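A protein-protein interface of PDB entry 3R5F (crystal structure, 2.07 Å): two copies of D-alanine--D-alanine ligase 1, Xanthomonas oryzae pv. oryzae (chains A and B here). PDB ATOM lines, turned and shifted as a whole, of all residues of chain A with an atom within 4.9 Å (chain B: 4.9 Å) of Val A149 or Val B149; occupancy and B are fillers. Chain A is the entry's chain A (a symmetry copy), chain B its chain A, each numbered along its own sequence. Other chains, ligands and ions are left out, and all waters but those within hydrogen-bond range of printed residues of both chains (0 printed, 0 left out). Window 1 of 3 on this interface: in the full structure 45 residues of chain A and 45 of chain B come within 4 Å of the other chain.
Among the printed residues, merely in contact across the chains: Gly A131 with Val B149 (3.96 Å), Ser A132 with Val B149 (3.8 Å), Val A149 with Gly B131 (3.96 Å), Val A149 with Ser B132 (3.8 Å), Val A149 with Val B149 (3.5 Å), Leu A150 with Ala B153 (3.6 Å), Leu A150 with Val B154 (3.8 Å), Ala A153 with Leu B150 (3.6 Å), Val A154 with Leu B150 (3.8 Å) and Val A154 with Val B154 (3.7 Å).
Of the 14 printed residues of chain A, 9 touch a printed residue of chain B. Along chain A the printed residues that touch a printed residue of chain B span positions 130 to 154. Of the 14 printed residues of chain B, 9 touch a printed residue of chain A. Among the printed residues, 16 pairs touch across the chains.
Of the printed residues of chain B, Asp A130 touches Arg B138. Val A149 touches just these residues of chain B: Gly B131 (3.96 Å), Ser B132 (3.8 Å) and Val B149 (3.5 Å). Of chain A, only Gly A131, Ser A132 and Val A149 come within 4 Å of Val B149. Of the printed residues of chain A, Val B154 touches Leu A150 and Val A154. The nearest residue of chain B that does not touch Val A149 is Asp B130 (4.1 Å).
Asp A130 touches Arg B138, and with the chains exchanged Arg A138 touches Asp B130. Ser A132 touches Gly B135, and with the chains exchanged Gly A135 touches Ser B132. Val A149 touches its own counterpart, Val B149. Val B154 touches its own counterpart, Val A154. Positions printed for both chains: 130, 131, 132, 134, 135, 138, 147, 148, 149, 150, 151, 152, 153 and 154. Of the 16 pairs that touch across the chains among the printed residues, 16 have their exchanged pair printed and touching as well.
The guanidinium group (NE) of Arg B138 sits at hydrogen-bond distance from the side-chain hydroxyl (OG) of Ser A132, at 2.9 Å. The backbone carbonyl oxygen of Gly A135 lies close to the backbone carbonyl oxygen of Ser B132. The side-chain carboxylate (OD2) of Asp A130 lies within salt-bridge range of the guanidinium group (NH2) of Arg B138 (2.9 Å). The side-chain hydroxyl of Ser B132 lies within hydrogen-bond range of the guanidinium group of Arg A138. The side-chain carboxylate (OD2) of Asp B130 lies within salt-bridge range of the guanidinium group (NH2) of Arg A138. The backbone carbonyl oxygen of Ser A132 lies close to the backbone carbonyl oxygen of Gly B135, at 3.4 Å.
The backbone NH of Gly A131 lies close to the side-chain amide oxygen of Gln A134, at 3.0 Å. The backbone carbonyl oxygen (O) of Asp A130 lies close to the backbone NH (N) of Ala A153 (3.5 Å). N of Ala B153 lies close to O of Asp B130, 3.5 Å away. The side-chain carboxylate of Asp A130 lies within hydrogen-bond range of the side-chain hydroxyl of Ser A132, at 2.6 Å. The side-chain amide oxygen (OE1) of Gln B134 sits close to the backbone NH (N) of Gly B131, 3.0 Å away. OG of Ser B132 sits at hydrogen-bond distance from OD1 of Asp B130, at 2.6 Å.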
ATOM      1  N   ASP A 130      29.880  28.064   0.489  1.00  0.00           N
ATOM      2  CA  ASP A 130      28.950  27.258  -0.292  1.00  0.00           C
ATOM      3  C   ASP A 130      29.048  25.774   0.014  1.00  0.00           C
ATOM      4  O   ASP A 130      28.386  24.982  -0.654  1.00  0.00           O
ATOM      5  CB  ASP A 130      29.064  27.533  -1.824  1.00  0.00           C
ATOM      6  CG  ASP A 130      30.276  26.937  -2.455  1.00  0.00           C
ATOM      7  OD1 ASP A 130      31.162  26.359  -1.760  1.00  0.00           O
ATOM      8  OD2 ASP A 130      30.398  27.061  -3.705  1.00  0.00           O
ATOM      9  N   GLY A 131      29.855  25.401   1.019  1.00  0.00           N
ATOM     10  CA  GLY A 131      29.992  23.966   1.356  1.00  0.00           C
ATOM     11  C   GLY A 131      31.333  23.394   0.934  1.00  0.00           C
ATOM     12  O   GLY A 131      31.697  22.281   1.395  1.00  0.00           O
ATOM     13  N   SER A 132      32.054  24.098   0.036  1.00  0.00           N
ATOM     14  CA  SER A 132      33.310  23.567  -0.496  1.00  0.00           C
ATOM     15  C   SER A 132      34.360  23.541   0.603  1.00  0.00           C
ATOM     16  O   SER A 132      35.062  22.520   0.822  1.00  0.00           O
ATOM     17  CB  SER A 132      33.830  24.430  -1.683  1.00  0.00           C
ATOM     18  OG  SER A 132      32.793  24.529  -2.675  1.00  0.00           O
ATOM     19  N   GLN A 134      33.844  23.595   3.761  1.00  0.00           N
ATOM     20  CA  GLN A 134      33.302  22.634   4.720  1.00  0.00           C
ATOM     21  C   GLN A 134      33.646  21.189   4.321  1.00  0.00           C
ATOM     22  O   GLN A 134      34.002  20.307   5.205  1.00  0.00           O
ATOM     23  CB  GLN A 134      31.764  22.841   4.845  1.00  0.00           C
ATOM     24  CG  GLN A 134      31.359  24.155   5.575  1.00  0.00           C
ATOM     25  CD  GLN A 134      31.555  25.394   4.719  1.00  0.00           C
ATOM     26  OE1 GLN A 134      31.600  25.327   3.477  1.00  0.00           O
ATOM     27  NE2 GLN A 134      31.670  26.534   5.373  1.00  0.00           N
ATOM     28  N   GLY A 135      33.613  20.944   3.010  1.00  0.00           N
ATOM     29  CA  GLY A 135      33.928  19.601   2.556  1.00  0.00           C
ATOM     30  C   GLY A 135      35.399  19.227   2.698  1.00  0.00           C
ATOM     31  O   GLY A 135      35.731  18.086   3.029  1.00  0.00           O
ATOM     32  N   ARG A 138      35.798  18.487   6.345  1.00  0.00           N
ATOM     33  CA  ARG A 138      35.353  17.094   6.504  1.00  0.00           C
ATOM     34  C   ARG A 138      36.359  16.037   6.027  1.00  0.00           C
ATOM     35  O   ARG A 138      36.467  14.962   6.657  1.00  0.00           O
ATOM     36  CB  ARG A 138      34.010  16.815   5.823  1.00  0.00           C
ATOM     37  CG  ARG A 138      32.860  17.128   6.779  1.00  0.00           C
ATOM     38  CD  ARG A 138      31.566  17.001   6.082  1.00  0.00           C
ATOM     39  NE  ARG A 138      31.164  15.617   5.757  1.00  0.00           N
ATOM     40  CZ  ARG A 138      30.581  14.769   6.588  1.00  0.00           C
ATOM     41  NH1 ARG A 138      30.343  15.087   7.857  1.00  0.00           N
ATOM     42  NH2 ARG A 138      30.241  13.591   6.148  1.00  0.00           N
ATOM     43  N   SER A 147      27.468  25.586   9.676  1.00  0.00           N
ATOM     44  CA  SER A 147      26.824  24.515   8.916  1.00  0.00           C
ATOM     45  C   SER A 147      27.788  23.528   8.214  1.00  0.00           C
ATOM     46  O   SER A 147      28.903  23.878   7.843  1.00  0.00           O
ATOM     47  CB  SER A 147      25.756  25.069   7.978  1.00  0.00           C
ATOM     48  OG  SER A 147      24.858  25.910   8.716  1.00  0.00           O
ATOM     49  N   GLY A 148      27.311  22.305   8.042  1.00  0.00           N
ATOM     50  CA  GLY A 148      28.076  21.267   7.378  1.00  0.00           C
ATOM     51  C   GLY A 148      27.914  21.442   5.876  1.00  0.00           C
ATOM     52  O   GLY A 148      27.478  22.500   5.425  1.00  0.00           O
ATOM     53  N   VAL A 149      28.247  20.418   5.121  1.00  0.00           N
ATOM     54  CA  VAL A 149      28.272  20.618   3.627  1.00  0.00           C
ATOM     55  C   VAL A 149      26.903  20.962   3.046  1.00  0.00           C
ATOM     56  O   VAL A 149      26.737  21.998   2.331  1.00  0.00           O
ATOM     57  CB  VAL A 149      28.960  19.397   2.951  1.00  0.00           C
ATOM     58  CG1 VAL A 149      28.999  19.538   1.415  1.00  0.00           C
ATOM     59  CG2 VAL A 149      30.429  19.283   3.535  1.00  0.00           C
ATOM     60  N   LEU A 150      25.911  20.113   3.347  1.00  0.00           N
ATOM     61  CA  LEU A 150      24.570  20.290   2.888  1.00  0.00           C
ATOM     62  C   LEU A 150      23.934  21.602   3.307  1.00  0.00           C
ATOM     63  O   LEU A 150      23.336  22.291   2.469  1.00  0.00           O
ATOM     64  CB  LEU A 150      23.665  19.088   3.304  1.00  0.00           C
ATOM     65  CG  LEU A 150      22.153  19.127   2.921  1.00  0.00           C
ATOM     66  CD1 LEU A 150      21.910  18.944   1.429  1.00  0.00           C
ATOM     67  CD2 LEU A 150      21.349  18.014   3.628  1.00  0.00           C
ATOM     68  N   GLY A 151      23.947  21.927   4.607  1.00  0.00           N
ATOM     69  CA  GLY A 151      23.285  23.133   5.072  1.00  0.00           C
ATOM     70  C   GLY A 151      23.892  24.380   4.423  1.00  0.00           C
ATOM     71  O   GLY A 151      23.167  25.358   4.137  1.00  0.00           O
ATOM     72  N   SER A 152      25.213  24.374   4.231  1.00  0.00           N
ATOM     73  CA  SER A 152      25.875  25.531   3.647  1.00  0.00           C
ATOM     74  C   SER A 152      25.504  25.643   2.161  1.00  0.00           C
ATOM     75  O   SER A 152      25.103  26.690   1.752  1.00  0.00           O
ATOM     76  CB  SER A 152      27.390  25.473   3.777  1.00  0.00           C
ATOM     77  OG  SER A 152      27.785  25.365   5.155  1.00  0.00           O
ATOM     78  N   ALA A 153      25.615  24.536   1.421  1.00  0.00           N
ATOM     79  CA  ALA A 153      25.332  24.488  -0.021  1.00  0.00           C
ATOM     80  C   ALA A 153      23.905  24.920  -0.200  1.00  0.00           C
ATOM     81  O   ALA A 153      23.585  25.688  -1.111  1.00  0.00           O
ATOM     82  CB  ALA A 153      25.503  23.017  -0.545  1.00  0.00           C
ATOM     83  N   VAL A 154      23.011  24.355   0.623  1.00  0.00           N
ATOM     84  CA  VAL A 154      21.567  24.604   0.388  1.00  0.00           C
ATOM     85  C   VAL A 154      21.216  26.070   0.705  1.00  0.00           C
ATOM     86  O   VAL A 154      20.511  26.744  -0.105  1.00  0.00           O
ATOM     87  CB  VAL A 154      20.648  23.621   1.154  1.00  0.00           C
ATOM     88  CG1 VAL A 154      19.262  24.165   1.045  1.00  0.00           C
ATOM     89  CG2 VAL A 154      20.616  22.266   0.442  1.00  0.00           C
ATOM     90  N   ASP B 130      28.957  12.599  -0.708  1.00  0.00           N
ATOM     91  CA  ASP B 130      28.025  13.528  -0.082  1.00  0.00           C
ATOM     92  C   ASP B 130      28.365  14.983  -0.351  1.00  0.00           C
ATOM     93  O   ASP B 130      27.712  15.862   0.208  1.00  0.00           O
ATOM     94  CB  ASP B 130      27.849  13.258   1.445  1.00  0.00           C
ATOM     95  CG  ASP B 130      29.008  13.696   2.274  1.00  0.00           C
ATOM     96  OD1 ASP B 130      30.064  14.146   1.739  1.00  0.00           O
ATOM     97  OD2 ASP B 130      28.906  13.572   3.525  1.00  0.00           O
ATOM     98  N   GLY B 131      29.368  15.237  -1.206  1.00  0.00           N
ATOM     99  CA  GLY B 131      29.745  16.638  -1.500  1.00  0.00           C
ATOM    100  C   GLY B 131      31.062  17.034  -0.858  1.00  0.00           C
ATOM    101  O   GLY B 131      31.639  18.085  -1.240  1.00  0.00           O
ATOM    102  N   SER B 132      31.527  16.252   0.139  1.00  0.00           N
ATOM    103  CA  SER B 132      32.737  16.619   0.877  1.00  0.00           C
ATOM    104  C   SER B 132      33.947  16.496  -0.035  1.00  0.00           C
ATOM    105  O   SER B 132      34.803  17.414  -0.124  1.00  0.00           O
ATOM    106  CB  SER B 132      32.937  15.709   2.124  1.00  0.00           C
ATOM    107  OG  SER B 132      31.748  15.757   2.930  1.00  0.00           O
ATOM    108  N   GLN B 134      33.955  16.476  -3.235  1.00  0.00           N
ATOM    109  CA  GLN B 134      33.708  17.489  -4.260  1.00  0.00           C
ATOM    110  C   GLN B 134      34.167  18.880  -3.794  1.00  0.00           C
ATOM    111  O   GLN B 134      34.777  19.699  -4.598  1.00  0.00           O
ATOM    112  CB  GLN B 134      32.198  17.484  -4.638  1.00  0.00           C
ATOM    113  CG  GLN B 134      31.750  16.226  -5.439  1.00  0.00           C
ATOM    114  CD  GLN B 134      31.639  14.981  -4.576  1.00  0.00           C
ATOM    115  OE1 GLN B 134      31.488  15.055  -3.342  1.00  0.00           O
ATOM    116  NE2 GLN B 134      31.710  13.829  -5.214  1.00  0.00           N
ATOM    117  N   GLY B 135      33.952  19.142  -2.504  1.00  0.00           N
ATOM    118  CA  GLY B 135      34.362  20.438  -1.990  1.00  0.00           C
ATOM    119  C   GLY B 135      35.871  20.614  -1.884  1.00  0.00           C
ATOM    120  O   GLY B 135      36.400  21.698  -2.143  1.00  0.00           O
ATOM    121  N   ARG B 138      36.957  21.256  -5.408  1.00  0.00           N
ATOM    122  CA  ARG B 138      36.731  22.693  -5.622  1.00  0.00           C
ATOM    123  C   ARG B 138      37.774  23.615  -4.975  1.00  0.00           C
ATOM    124  O   ARG B 138      38.123  24.660  -5.567  1.00  0.00           O
ATOM    125  CB  ARG B 138      35.342  23.153  -5.168  1.00  0.00           C
ATOM    126  CG  ARG B 138      34.334  22.983  -6.302  1.00  0.00           C
ATOM    127  CD  ARG B 138      32.971  23.285  -5.827  1.00  0.00           C
ATOM    128  NE  ARG B 138      32.706  24.713  -5.558  1.00  0.00           N
ATOM    129  CZ  ARG B 138      32.382  25.622  -6.464  1.00  0.00           C
ATOM    130  NH1 ARG B 138      32.317  25.323  -7.759  1.00  0.00           N
ATOM    131  NH2 ARG B 138      32.132  26.838  -6.074  1.00  0.00           N
ATOM    132  N   SER B 147      28.433  15.272 -10.139  1.00  0.00           N
ATOM    133  CA  SER B 147      27.819  16.425  -9.483  1.00  0.00           C
ATOM    134  C   SER B 147      28.774  17.285  -8.621  1.00  0.00           C
ATOM    135  O   SER B 147      29.758  16.797  -8.077  1.00  0.00           O
ATOM    136  CB  SER B 147      26.547  16.026  -8.740  1.00  0.00           C
ATOM    137  OG  SER B 147      25.680  15.301  -9.624  1.00  0.00           O
ATOM    138  N   GLY B 148      28.440  18.562  -8.517  1.00  0.00           N
ATOM    139  CA  GLY B 148      29.214  19.498  -7.726  1.00  0.00           C
ATOM    140  C   GLY B 148      28.786  19.363  -6.273  1.00  0.00           C
ATOM    141  O   GLY B 148      28.147  18.376  -5.911  1.00  0.00           O
ATOM    142  N   VAL B 149      29.121  20.342  -5.462  1.00  0.00           N
ATOM    143  CA  VAL B 149      28.874  20.156  -3.986  1.00  0.00           C
ATOM    144  C   VAL B 149      27.395  20.000  -3.642  1.00  0.00           C
ATOM    145  O   VAL B 149      26.980  19.003  -2.976  1.00  0.00           O
ATOM    146  CB  VAL B 149      29.595  21.285  -3.193  1.00  0.00           C
ATOM    147  CG1 VAL B 149      29.362  21.156  -1.673  1.00  0.00           C
ATOM    148  CG2 VAL B 149      31.142  21.200  -3.527  1.00  0.00           C
ATOM    149  N   LEU B 150      26.585  20.969  -4.092  1.00  0.00           N
ATOM    150  CA  LEU B 150      25.175  20.973  -3.861  1.00  0.00           C
ATOM    151  C   LEU B 150      24.451  19.751  -4.393  1.00  0.00           C
ATOM    152  O   LEU B 150      23.639  19.156  -3.673  1.00  0.00           O
ATOM    153  CB  LEU B 150      24.516  22.279  -4.408  1.00  0.00           C
ATOM    154  CG  LEU B 150      22.970  22.443  -4.280  1.00  0.00           C
ATOM    155  CD1 LEU B 150      22.511  22.672  -2.845  1.00  0.00           C
ATOM    156  CD2 LEU B 150      22.446  23.643  -5.097  1.00  0.00           C
ATOM    157  N   GLY B 151      24.635  19.414  -5.677  1.00  0.00           N
ATOM    158  CA  GLY B 151      23.907  18.300  -6.258  1.00  0.00           C
ATOM    159  C   GLY B 151      24.231  16.991  -5.533  1.00  0.00           C
ATOM    160  O   GLY B 151      23.347  16.119  -5.379  1.00  0.00           O
ATOM    161  N   SER B 152      25.491  16.826  -5.126  1.00  0.00           N
ATOM    162  CA  SER B 152      25.892  15.599  -4.454  1.00  0.00           C
ATOM    163  C   SER B 152      25.270  15.553  -3.049  1.00  0.00           C
ATOM    164  O   SER B 152      24.674  14.572  -2.724  1.00  0.00           O
ATOM    165  CB  SER B 152      27.402  15.458  -4.332  1.00  0.00           C
ATOM    166  OG  SER B 152      28.029  15.497  -5.625  1.00  0.00           O
ATOM    167  N   ALA B 153      25.402  16.644  -2.289  1.00  0.00           N
ATOM    168  CA  ALA B 153      24.894  16.744  -0.913  1.00  0.00           C
ATOM    169  C   ALA B 153      23.414  16.504  -0.975  1.00  0.00           C
ATOM    170  O   ALA B 153      22.850  15.795  -0.139  1.00  0.00           O
ATOM    171  CB  ALA B 153      25.167  18.185  -0.351  1.00  0.00           C
ATOM    172  N   VAL B 154      22.748  17.172  -1.928  1.00  0.00           N
ATOM    173  CA  VAL B 154      21.265  17.117  -1.936  1.00  0.00           C
ATOM    174  C   VAL B 154      20.783  15.705  -2.323  1.00  0.00           C
ATOM    175  O   VAL B 154      19.872  15.138  -1.647  1.00  0.00           O
ATOM    176  CB  VAL B 154      20.621  18.203  -2.833  1.00  0.00           C
ATOM    177  CG1 VAL B 154      19.177  17.845  -2.959  1.00  0.00           C
ATOM    178  CG2 VAL B 154      20.650  19.559  -2.121  1.00  0.00           C
